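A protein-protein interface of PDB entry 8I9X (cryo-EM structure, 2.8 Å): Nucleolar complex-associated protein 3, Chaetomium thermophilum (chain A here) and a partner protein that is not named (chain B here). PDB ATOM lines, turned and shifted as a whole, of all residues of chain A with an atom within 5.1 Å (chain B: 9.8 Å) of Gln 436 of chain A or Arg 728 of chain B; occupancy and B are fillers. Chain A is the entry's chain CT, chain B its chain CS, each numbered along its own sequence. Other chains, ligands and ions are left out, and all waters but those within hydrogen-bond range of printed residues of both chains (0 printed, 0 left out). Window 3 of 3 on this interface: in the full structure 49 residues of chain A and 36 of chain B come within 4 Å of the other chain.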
ATOM      1  N   ILE A 434     -22.932  21.861  -0.451  1.00  0.00           N
ATOM      2  CA  ILE A 434     -22.811  21.934  -1.907  1.00  0.00           C
ATOM      3  C   ILE A 434     -24.202  21.996  -2.530  1.00  0.00           C
ATOM      4  O   ILE A 434     -25.212  21.837  -1.836  1.00  0.00           O
ATOM      5  CB  ILE A 434     -22.010  20.764  -2.502  1.00  0.00           C
ATOM      6  CG1 ILE A 434     -22.783  19.455  -2.360  1.00  0.00           C
ATOM      7  CG2 ILE A 434     -20.646  20.690  -1.859  1.00  0.00           C
ATOM      8  CD1 ILE A 434     -22.237  18.334  -3.208  1.00  0.00           C
ATOM      9  N   ASN A 435     -24.256  22.248  -3.837  1.00  0.00           N
ATOM     10  CA  ASN A 435     -25.518  22.504  -4.522  1.00  0.00           C
ATOM     11  C   ASN A 435     -26.435  21.285  -4.520  1.00  0.00           C
ATOM     12  O   ASN A 435     -26.113  20.233  -3.960  1.00  0.00           O
ATOM     13  CB  ASN A 435     -25.263  22.946  -5.964  1.00  0.00           C
ATOM     14  CG  ASN A 435     -24.718  24.354  -6.056  1.00  0.00           C
ATOM     15  OD1 ASN A 435     -25.083  25.225  -5.271  1.00  0.00           O
ATOM     16  ND2 ASN A 435     -23.843  24.586  -7.027  1.00  0.00           N
ATOM     17  N   GLN A 436     -27.587  21.442  -5.176  1.00  0.00           N
ATOM     18  CA  GLN A 436     -28.723  20.552  -4.964  1.00  0.00           C
ATOM     19  C   GLN A 436     -28.734  19.409  -5.980  1.00  0.00           C
ATOM     20  O   GLN A 436     -28.774  18.218  -5.617  1.00  0.00           O
ATOM     21  CB  GLN A 436     -29.997  21.391  -5.053  1.00  0.00           C
ATOM     22  CG  GLN A 436     -31.142  20.950  -4.191  1.00  0.00           C
ATOM     23  CD  GLN A 436     -32.248  21.985  -4.149  1.00  0.00           C
ATOM     24  OE1 GLN A 436     -32.186  23.001  -4.838  1.00  0.00           O
ATOM     25  NE2 GLN A 436     -33.268  21.731  -3.338  1.00  0.00           N
ATOM     26  N   ASP A 437     -28.704  19.755  -7.270  1.00  0.00           N
ATOM     27  CA  ASP A 437     -28.551  18.738  -8.300  1.00  0.00           C
ATOM     28  C   ASP A 437     -27.314  17.892  -8.057  1.00  0.00           C
ATOM     29  O   ASP A 437     -27.320  16.692  -8.353  1.00  0.00           O
ATOM     30  CB  ASP A 437     -28.486  19.388  -9.682  1.00  0.00           C
ATOM     31  CG  ASP A 437     -27.423  20.466  -9.771  1.00  0.00           C
ATOM     32  OD1 ASP A 437     -26.811  20.789  -8.732  1.00  0.00           O
ATOM     33  OD2 ASP A 437     -27.197  20.989 -10.882  1.00  0.00           O
ATOM     34  N   PHE A 438     -26.267  18.481  -7.492  1.00  0.00           N
ATOM     35  CA  PHE A 438     -25.113  17.732  -7.031  1.00  0.00           C
ATOM     36  C   PHE A 438     -25.451  16.778  -5.896  1.00  0.00           C
ATOM     37  O   PHE A 438     -24.845  15.712  -5.809  1.00  0.00           O
ATOM     38  CB  PHE A 438     -24.000  18.691  -6.604  1.00  0.00           C
ATOM     39  CG  PHE A 438     -23.500  19.567  -7.716  1.00  0.00           C
ATOM     40  CD1 PHE A 438     -23.687  19.203  -9.038  1.00  0.00           C
ATOM     41  CD2 PHE A 438     -22.852  20.755  -7.441  1.00  0.00           C
ATOM     42  CE1 PHE A 438     -23.235  20.006 -10.063  1.00  0.00           C
ATOM     43  CE2 PHE A 438     -22.398  21.562  -8.465  1.00  0.00           C
ATOM     44  CZ  PHE A 438     -22.589  21.185  -9.776  1.00  0.00           C
ATOM     45  N   PHE A 439     -26.403  17.125  -5.027  1.00  0.00           N
ATOM     46  CA  PHE A 439     -26.835  16.171  -4.010  1.00  0.00           C
ATOM     47  C   PHE A 439     -27.449  14.936  -4.655  1.00  0.00           C
ATOM     48  O   PHE A 439     -27.111  13.795  -4.293  1.00  0.00           O
ATOM     49  CB  PHE A 439     -27.831  16.835  -3.058  1.00  0.00           C
ATOM     50  CG  PHE A 439     -27.895  16.202  -1.704  1.00  0.00           C
ATOM     51  CD1 PHE A 439     -28.676  15.083  -1.483  1.00  0.00           C
ATOM     52  CD2 PHE A 439     -27.179  16.731  -0.646  1.00  0.00           C
ATOM     53  CE1 PHE A 439     -28.738  14.501  -0.234  1.00  0.00           C
ATOM     54  CE2 PHE A 439     -27.237  16.154   0.605  1.00  0.00           C
ATOM     55  CZ  PHE A 439     -28.017  15.038   0.812  1.00  0.00           C
ATOM     56  N   GLY A 440     -28.323  15.145  -5.640  1.00  0.00           N
ATOM     57  CA  GLY A 440     -28.783  13.999  -6.412  1.00  0.00           C
ATOM     58  C   GLY A 440     -27.663  13.225  -7.085  1.00  0.00           C
ATOM     59  O   GLY A 440     -27.662  11.985  -7.054  1.00  0.00           O
ATOM     60  N   ALA A 501     -35.978  18.376   1.714  1.00  0.00           N
ATOM     61  CA  ALA A 501     -35.857  18.459   0.258  1.00  0.00           C
ATOM     62  C   ALA A 501     -36.434  17.221  -0.425  1.00  0.00           C
ATOM     63  O   ALA A 501     -36.762  17.255  -1.611  1.00  0.00           O
ATOM     64  CB  ALA A 501     -34.392  18.665  -0.133  1.00  0.00           C
ATOM     65  N   LEU A 505     -36.684  17.014  -4.453  1.00  0.00           N
ATOM     66  CA  LEU A 505     -35.420  16.585  -5.030  1.00  0.00           C
ATOM     67  C   LEU A 505     -35.440  15.152  -5.536  1.00  0.00           C
ATOM     68  O   LEU A 505     -34.468  14.721  -6.164  1.00  0.00           O
ATOM     69  CB  LEU A 505     -34.305  16.742  -4.001  1.00  0.00           C
ATOM     70  CG  LEU A 505     -33.491  18.025  -4.033  1.00  0.00           C
ATOM     71  CD1 LEU A 505     -32.293  17.863  -3.117  1.00  0.00           C
ATOM     72  CD2 LEU A 505     -33.060  18.309  -5.454  1.00  0.00           C
ATOM     73  N   LYS B 719     -22.606  31.303 -17.772  1.00  0.00           N
ATOM     74  CA  LYS B 719     -23.183  31.368 -16.435  1.00  0.00           C
ATOM     75  C   LYS B 719     -23.036  30.056 -15.678  1.00  0.00           C
ATOM     76  O   LYS B 719     -22.694  30.073 -14.490  1.00  0.00           O
ATOM     77  CB  LYS B 719     -24.659  31.762 -16.506  1.00  0.00           C
ATOM     78  CG  LYS B 719     -24.900  33.176 -16.995  1.00  0.00           C
ATOM     79  CD  LYS B 719     -26.381  33.515 -16.989  1.00  0.00           C
ATOM     80  CE  LYS B 719     -26.629  34.905 -17.555  1.00  0.00           C
ATOM     81  NZ  LYS B 719     -26.079  35.969 -16.671  1.00  0.00           N
ATOM     82  N   ARG B 723     -20.786  29.599 -12.333  1.00  0.00           N
ATOM     83  CA  ARG B 723     -21.614  29.424 -11.147  1.00  0.00           C
ATOM     84  C   ARG B 723     -20.770  28.884  -9.998  1.00  0.00           C
ATOM     85  O   ARG B 723     -19.950  27.981 -10.189  1.00  0.00           O
ATOM     86  CB  ARG B 723     -22.778  28.476 -11.429  1.00  0.00           C
ATOM     87  CG  ARG B 723     -23.735  28.353 -10.254  1.00  0.00           C
ATOM     88  CD  ARG B 723     -24.901  27.421 -10.528  1.00  0.00           C
ATOM     89  NE  ARG B 723     -24.475  26.035 -10.673  1.00  0.00           N
ATOM     90  CZ  ARG B 723     -25.262  25.049 -11.080  1.00  0.00           C
ATOM     91  NH1 ARG B 723     -26.532  25.259 -11.386  1.00  0.00           N
ATOM     92  NH2 ARG B 723     -24.765  23.820 -11.177  1.00  0.00           N
ATOM     93  N   ALA B 724     -20.973  29.438  -8.806  1.00  0.00           N
ATOM     94  CA  ALA B 724     -20.247  28.985  -7.632  1.00  0.00           C
ATOM     95  C   ALA B 724     -20.731  27.604  -7.201  1.00  0.00           C
ATOM     96  O   ALA B 724     -21.847  27.180  -7.510  1.00  0.00           O
ATOM     97  CB  ALA B 724     -20.409  29.980  -6.483  1.00  0.00           C
ATOM     98  N   LEU B 725     -19.863  26.891  -6.480  1.00  0.00           N
ATOM     99  CA  LEU B 725     -20.220  25.553  -6.023  1.00  0.00           C
ATOM    100  C   LEU B 725     -21.232  25.596  -4.884  1.00  0.00           C
ATOM    101  O   LEU B 725     -22.014  24.654  -4.718  1.00  0.00           O
ATOM    102  CB  LEU B 725     -18.966  24.790  -5.601  1.00  0.00           C
ATOM    103  CG  LEU B 725     -19.211  23.334  -5.207  1.00  0.00           C
ATOM    104  CD1 LEU B 725     -19.787  22.583  -6.385  1.00  0.00           C
ATOM    105  CD2 LEU B 725     -17.940  22.670  -4.726  1.00  0.00           C
ATOM    106  N   ASN B 726     -21.242  26.671  -4.098  1.00  0.00           N
ATOM    107  CA  ASN B 726     -22.242  26.866  -3.057  1.00  0.00           C
ATOM    108  C   ASN B 726     -23.281  27.904  -3.460  1.00  0.00           C
ATOM    109  O   ASN B 726     -23.807  28.621  -2.603  1.00  0.00           O
ATOM    110  CB  ASN B 726     -21.577  27.266  -1.741  1.00  0.00           C
ATOM    111  CG  ASN B 726     -20.810  28.561  -1.848  1.00  0.00           C
ATOM    112  OD1 ASN B 726     -20.142  28.812  -2.845  1.00  0.00           O
ATOM    113  ND2 ASN B 726     -20.905  29.394  -0.820  1.00  0.00           N
ATOM    114  N   ALA B 727     -23.581  27.997  -4.756  1.00  0.00           N
ATOM    115  CA  ALA B 727     -24.507  29.015  -5.237  1.00  0.00           C
ATOM    116  C   ALA B 727     -25.940  28.718  -4.815  1.00  0.00           C
ATOM    117  O   ALA B 727     -26.661  29.621  -4.377  1.00  0.00           O
ATOM    118  CB  ALA B 727     -24.408  29.124  -6.756  1.00  0.00           C
ATOM    119  N   ARG B 728     -26.368  27.462  -4.921  1.00  0.00           N
ATOM    120  CA  ARG B 728     -27.753  27.071  -4.658  1.00  0.00           C
ATOM    121  C   ARG B 728     -27.795  25.937  -3.644  1.00  0.00           C
ATOM    122  O   ARG B 728     -28.100  24.790  -3.989  1.00  0.00           O
ATOM    123  CB  ARG B 728     -28.457  26.652  -5.949  1.00  0.00           C
ATOM    124  CG  ARG B 728     -28.417  27.686  -7.052  1.00  0.00           C
ATOM    125  CD  ARG B 728     -29.387  27.353  -8.177  1.00  0.00           C
ATOM    126  NE  ARG B 728     -30.635  26.779  -7.689  1.00  0.00           N
ATOM    127  CZ  ARG B 728     -30.993  25.513  -7.853  1.00  0.00           C
ATOM    128  NH1 ARG B 728     -30.221  24.655  -8.497  1.00  0.00           N
ATOM    129  NH2 ARG B 728     -32.157  25.099  -7.360  1.00  0.00           N
ATOM    130  N   PRO B 729     -27.495  26.219  -2.382  1.00  0.00           N
ATOM    131  CA  PRO B 729     -27.685  25.217  -1.335  1.00  0.00           C
ATOM    132  C   PRO B 729     -29.166  25.020  -1.038  1.00  0.00           C
ATOM    133  O   PRO B 729     -30.014  25.865  -1.338  1.00  0.00           O
ATOM    134  CB  PRO B 729     -26.950  25.806  -0.124  1.00  0.00           C
ATOM    135  CG  PRO B 729     -26.154  26.955  -0.656  1.00  0.00           C
ATOM    136  CD  PRO B 729     -26.902  27.451  -1.843  1.00  0.00           C
ATOM    137  N   ILE B 730     -29.462  23.868  -0.435  1.00  0.00           N
ATOM    138  CA  ILE B 730     -30.836  23.559  -0.060  1.00  0.00           C
ATOM    139  C   ILE B 730     -31.376  24.605   0.902  1.00  0.00           C
ATOM    140  O   ILE B 730     -32.526  25.040   0.774  1.00  0.00           O
ATOM    141  CB  ILE B 730     -30.918  22.146   0.543  1.00  0.00           C
ATOM    142  CG1 ILE B 730     -30.386  21.112  -0.450  1.00  0.00           C
ATOM    143  CG2 ILE B 730     -32.346  21.813   0.930  1.00  0.00           C
ATOM    144  CD1 ILE B 730     -30.082  19.776   0.173  1.00  0.00           C
ATOM    145  N   LYS B 731     -30.563  25.027   1.872  1.00  0.00           N
ATOM    146  CA  LYS B 731     -31.011  26.021   2.839  1.00  0.00           C
ATOM    147  C   LYS B 731     -31.365  27.338   2.158  1.00  0.00           C
ATOM    148  O   LYS B 731     -32.404  27.938   2.454  1.00  0.00           O
ATOM    149  CB  LYS B 731     -29.934  26.235   3.901  1.00  0.00           C
ATOM    150  CG  LYS B 731     -30.355  27.148   5.037  1.00  0.00           C
ATOM    151  CD  LYS B 731     -29.240  27.309   6.055  1.00  0.00           C
ATOM    152  CE  LYS B 731     -29.031  26.030   6.851  1.00  0.00           C
ATOM    153  NZ  LYS B 731     -30.197  25.723   7.727  1.00  0.00           N
ATOM    154  N   LYS B 732     -30.513  27.804   1.241  1.00  0.00           N
ATOM    155  CA  LYS B 732     -30.787  29.072   0.573  1.00  0.00           C
ATOM    156  C   LYS B 732     -31.998  28.982  -0.346  1.00  0.00           C
ATOM    157  O   LYS B 732     -32.803  29.919  -0.392  1.00  0.00           O
ATOM    158  CB  LYS B 732     -29.560  29.557  -0.197  1.00  0.00           C
ATOM    159  CG  LYS B 732     -28.392  29.940   0.698  1.00  0.00           C
ATOM    160  CD  LYS B 732     -27.210  30.449  -0.108  1.00  0.00           C
ATOM    161  CE  LYS B 732     -26.084  30.912   0.799  1.00  0.00           C
ATOM    162  NZ  LYS B 732     -25.479  29.779   1.553  1.00  0.00           N
ATOM    163  N   VAL B 733     -32.155  27.875  -1.075  1.00  0.00           N
ATOM    164  CA  VAL B 733     -33.353  27.728  -1.898  1.00  0.00           C
ATOM    165  C   VAL B 733     -34.608  27.711  -1.031  1.00  0.00           C
ATOM    166  O   VAL B 733     -35.604  28.380  -1.348  1.00  0.00           O
ATOM    167  CB  VAL B 733     -33.252  26.464  -2.772  1.00  0.00           C
ATOM    168  CG1 VAL B 733     -34.540  26.252  -3.548  1.00  0.00           C
ATOM    169  CG2 VAL B 733     -32.071  26.575  -3.722  1.00  0.00           C
ATOM    170  N   ALA B 734     -34.576  26.969   0.078  1.00  0.00           N
ATOM    171  CA  ALA B 734     -35.736  26.889   0.958  1.00  0.00           C
ATOM    172  C   ALA B 734     -36.074  28.249   1.552  1.00  0.00           C
ATOM    173  O   ALA B 734     -37.249  28.627   1.629  1.00  0.00           O
ATOM    174  CB  ALA B 734     -35.484  25.864   2.063  1.00  0.00           C
ATOM    175  N   GLU B 735     -35.061  29.006   1.981  1.00  0.00           N
ATOM    176  CA  GLU B 735     -35.339  30.306   2.573  1.00  0.00           C
ATOM    177  C   GLU B 735     -35.775  31.334   1.540  1.00  0.00           C
ATOM    178  O   GLU B 735     -36.564  32.220   1.874  1.00  0.00           O
ATOM    179  CB  GLU B 735     -34.126  30.823   3.352  1.00  0.00           C
ATOM    180  CG  GLU B 735     -32.905  31.133   2.519  1.00  0.00           C
ATOM    181  CD  GLU B 735     -31.719  31.558   3.363  1.00  0.00           C
ATOM    182  OE1 GLU B 735     -31.853  31.585   4.604  1.00  0.00           O
ATOM    183  OE2 GLU B 735     -30.655  31.863   2.786  1.00  0.00           O
ATOM    184  N   ALA B 736     -35.310  31.230   0.293  1.00  0.00           N
ATOM    185  CA  ALA B 736     -35.845  32.096  -0.754  1.00  0.00           C
ATOM    186  C   ALA B 736     -37.316  31.797  -1.015  1.00  0.00           C
ATOM    187  O   ALA B 736     -38.132  32.720  -1.164  1.00  0.00           O
ATOM    188  CB  ALA B 736     -35.026  31.939  -2.034  1.00  0.00           C
ATOM    189  N   ARG B 737     -37.676  30.510  -1.072  1.00  0.00           N
ATOM    190  CA  ARG B 737     -39.083  30.156  -1.223  1.00  0.00           C
ATOM    191  C   ARG B 737     -39.912  30.645  -0.041  1.00  0.00           C
ATOM    192  O   ARG B 737     -41.027  31.146  -0.229  1.00  0.00           O
ATOM    193  CB  ARG B 737     -39.234  28.644  -1.387  1.00  0.00           C
ATOM    194  CG  ARG B 737     -38.656  28.098  -2.679  1.00  0.00           C
ATOM    195  CD  ARG B 737     -38.874  26.597  -2.786  1.00  0.00           C
ATOM    196  NE  ARG B 737     -38.250  26.035  -3.977  1.00  0.00           N
ATOM    197  CZ  ARG B 737     -38.840  25.940  -5.160  1.00  0.00           C
ATOM    198  NH1 ARG B 737     -40.079  26.366  -5.350  1.00  0.00           N
ATOM    199  NH2 ARG B 737     -38.172  25.405  -6.178  1.00  0.00           N
ATOM    200  N   ARG B 740     -40.457  34.429  -0.451  1.00  0.00           N
ATOM    201  CA  ARG B 740     -41.486  34.789  -1.424  1.00  0.00           C
ATOM    202  C   ARG B 740     -42.882  34.425  -0.925  1.00  0.00           C
ATOM    203  O   ARG B 740     -43.842  35.167  -1.175  1.00  0.00           O
ATOM    204  CB  ARG B 740     -41.197  34.145  -2.785  1.00  0.00           C
ATOM    205  CG  ARG B 740     -41.436  32.651  -2.876  1.00  0.00           C
ATOM    206  CD  ARG B 740     -41.101  32.119  -4.262  1.00  0.00           C
ATOM    207  NE  ARG B 740     -39.674  32.199  -4.551  1.00  0.00           N
ATOM    208  CZ  ARG B 740     -39.133  33.038  -5.425  1.00  0.00           C
ATOM    209  NH1 ARG B 740     -39.874  33.888  -6.117  1.00  0.00           N
ATOM    210  NH2 ARG B 740     -37.816  33.022  -5.608  1.00  0.00           N
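Among the printed residues, pairs that only touch across the chains: Phe 438 of chain A with Leu 725 of chain B (3.5 Å), Phe 438 of chain A with Arg 723 of chain B (3.7 Å), Asn 435 of chain A with Asn 726 of chain B (3.7 Å), Gln 436 of chain A with Val 733 of chain B (3.7 Å), Gln 436 of chain A with Ile 730 of chain B (3.8 Å), Asn 435 of chain A with Pro 729 of chain B (3.9 Å), Ala 501 of chain A with Ile 730 of chain B (3.9 Å), Asn 435 of chain A with Arg 723 of chain B (3.97 Å) and Ile 434 of chain A with Leu 725 of chain B (3.99 Å).
Printed residues of chain B that touch a printed residue of chain A: Arg 723, Ala 724, Leu 725, Asn 726, Ala 727, Arg 728, Pro 729, Ile 730 and Val 733.
Hydrophobic or aromatic side chains of chain B within 4 Å of the printed part of chain A: Leu 725, Ile 730 and Val 733.
Printed residues of chain A that touch a printed residue of chain B: Ile 434, Asn 435, Gln 436, Asp 437, Phe 438 and Ala 501.
Among the printed residues, 15 pairs touch across the chains.
Asn 435 of chain A touches just these residues of chain B: Arg 723 (3.97 Å), Ala 724 (3.3 Å), Leu 725 (2.9 Å), Asn 726 (3.7 Å), Ala 727 (3.2 Å), Arg 728 (2.6 Å) and Pro 729 (3.9 Å).
Gln 436 of chain A touches just these residues of chain B: Arg 728 (3.3 Å), Ile 730 (3.8 Å) and Val 733 (3.7 Å).
Printed residues of chain A within 4 Å of Ala 724 of chain B: Asn 435 (3.3 Å).
Of the printed residues of chain A, Leu 725 of chain B touches Ile 434, Asn 435 and Phe 438.
Of the printed residues of chain A, Ala 727 of chain B touches Asn 435 (3.2 Å).
Of the printed residues of chain A, Arg 728 of chain B touches Asn 435 and Gln 436.
Printed residues of chain A within 4 Å of Pro 729 of chain B: Asn 435.
The backbone carbonyl oxygen (O) of Leu 725 of chain B is in hydrogen-bond range of the side-chain amide nitrogen (ND2) of Asn 435 of chain A (2.9 Å).
The backbone carbonyl oxygen (O) of Ala 724 of chain B lies within hydrogen-bond range of the side-chain amide nitrogen (ND2) of Asn 435 of chain A, 3.3 Å away.
NH2 of Arg 728 of chain B is in hydrogen-bond range of OE1 of Gln 436 of chain A (3.3 Å).
The backbone NH (N) of Ala 727 of chain B lies within hydrogen-bond range of the side-chain amide oxygen (OD1) of Asn 435 of chain A (3.2 Å).
The backbone NH of Arg 728 of chain B is in hydrogen-bond range of the side-chain amide oxygen of Asn 435 of chain A, 2.6 Å away.
The guanidinium group (NH2) of Arg 723 of chain B is in salt-bridge range of the side-chain carboxylate (OD2) of Asp 437 of chain A (3.7 Å).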
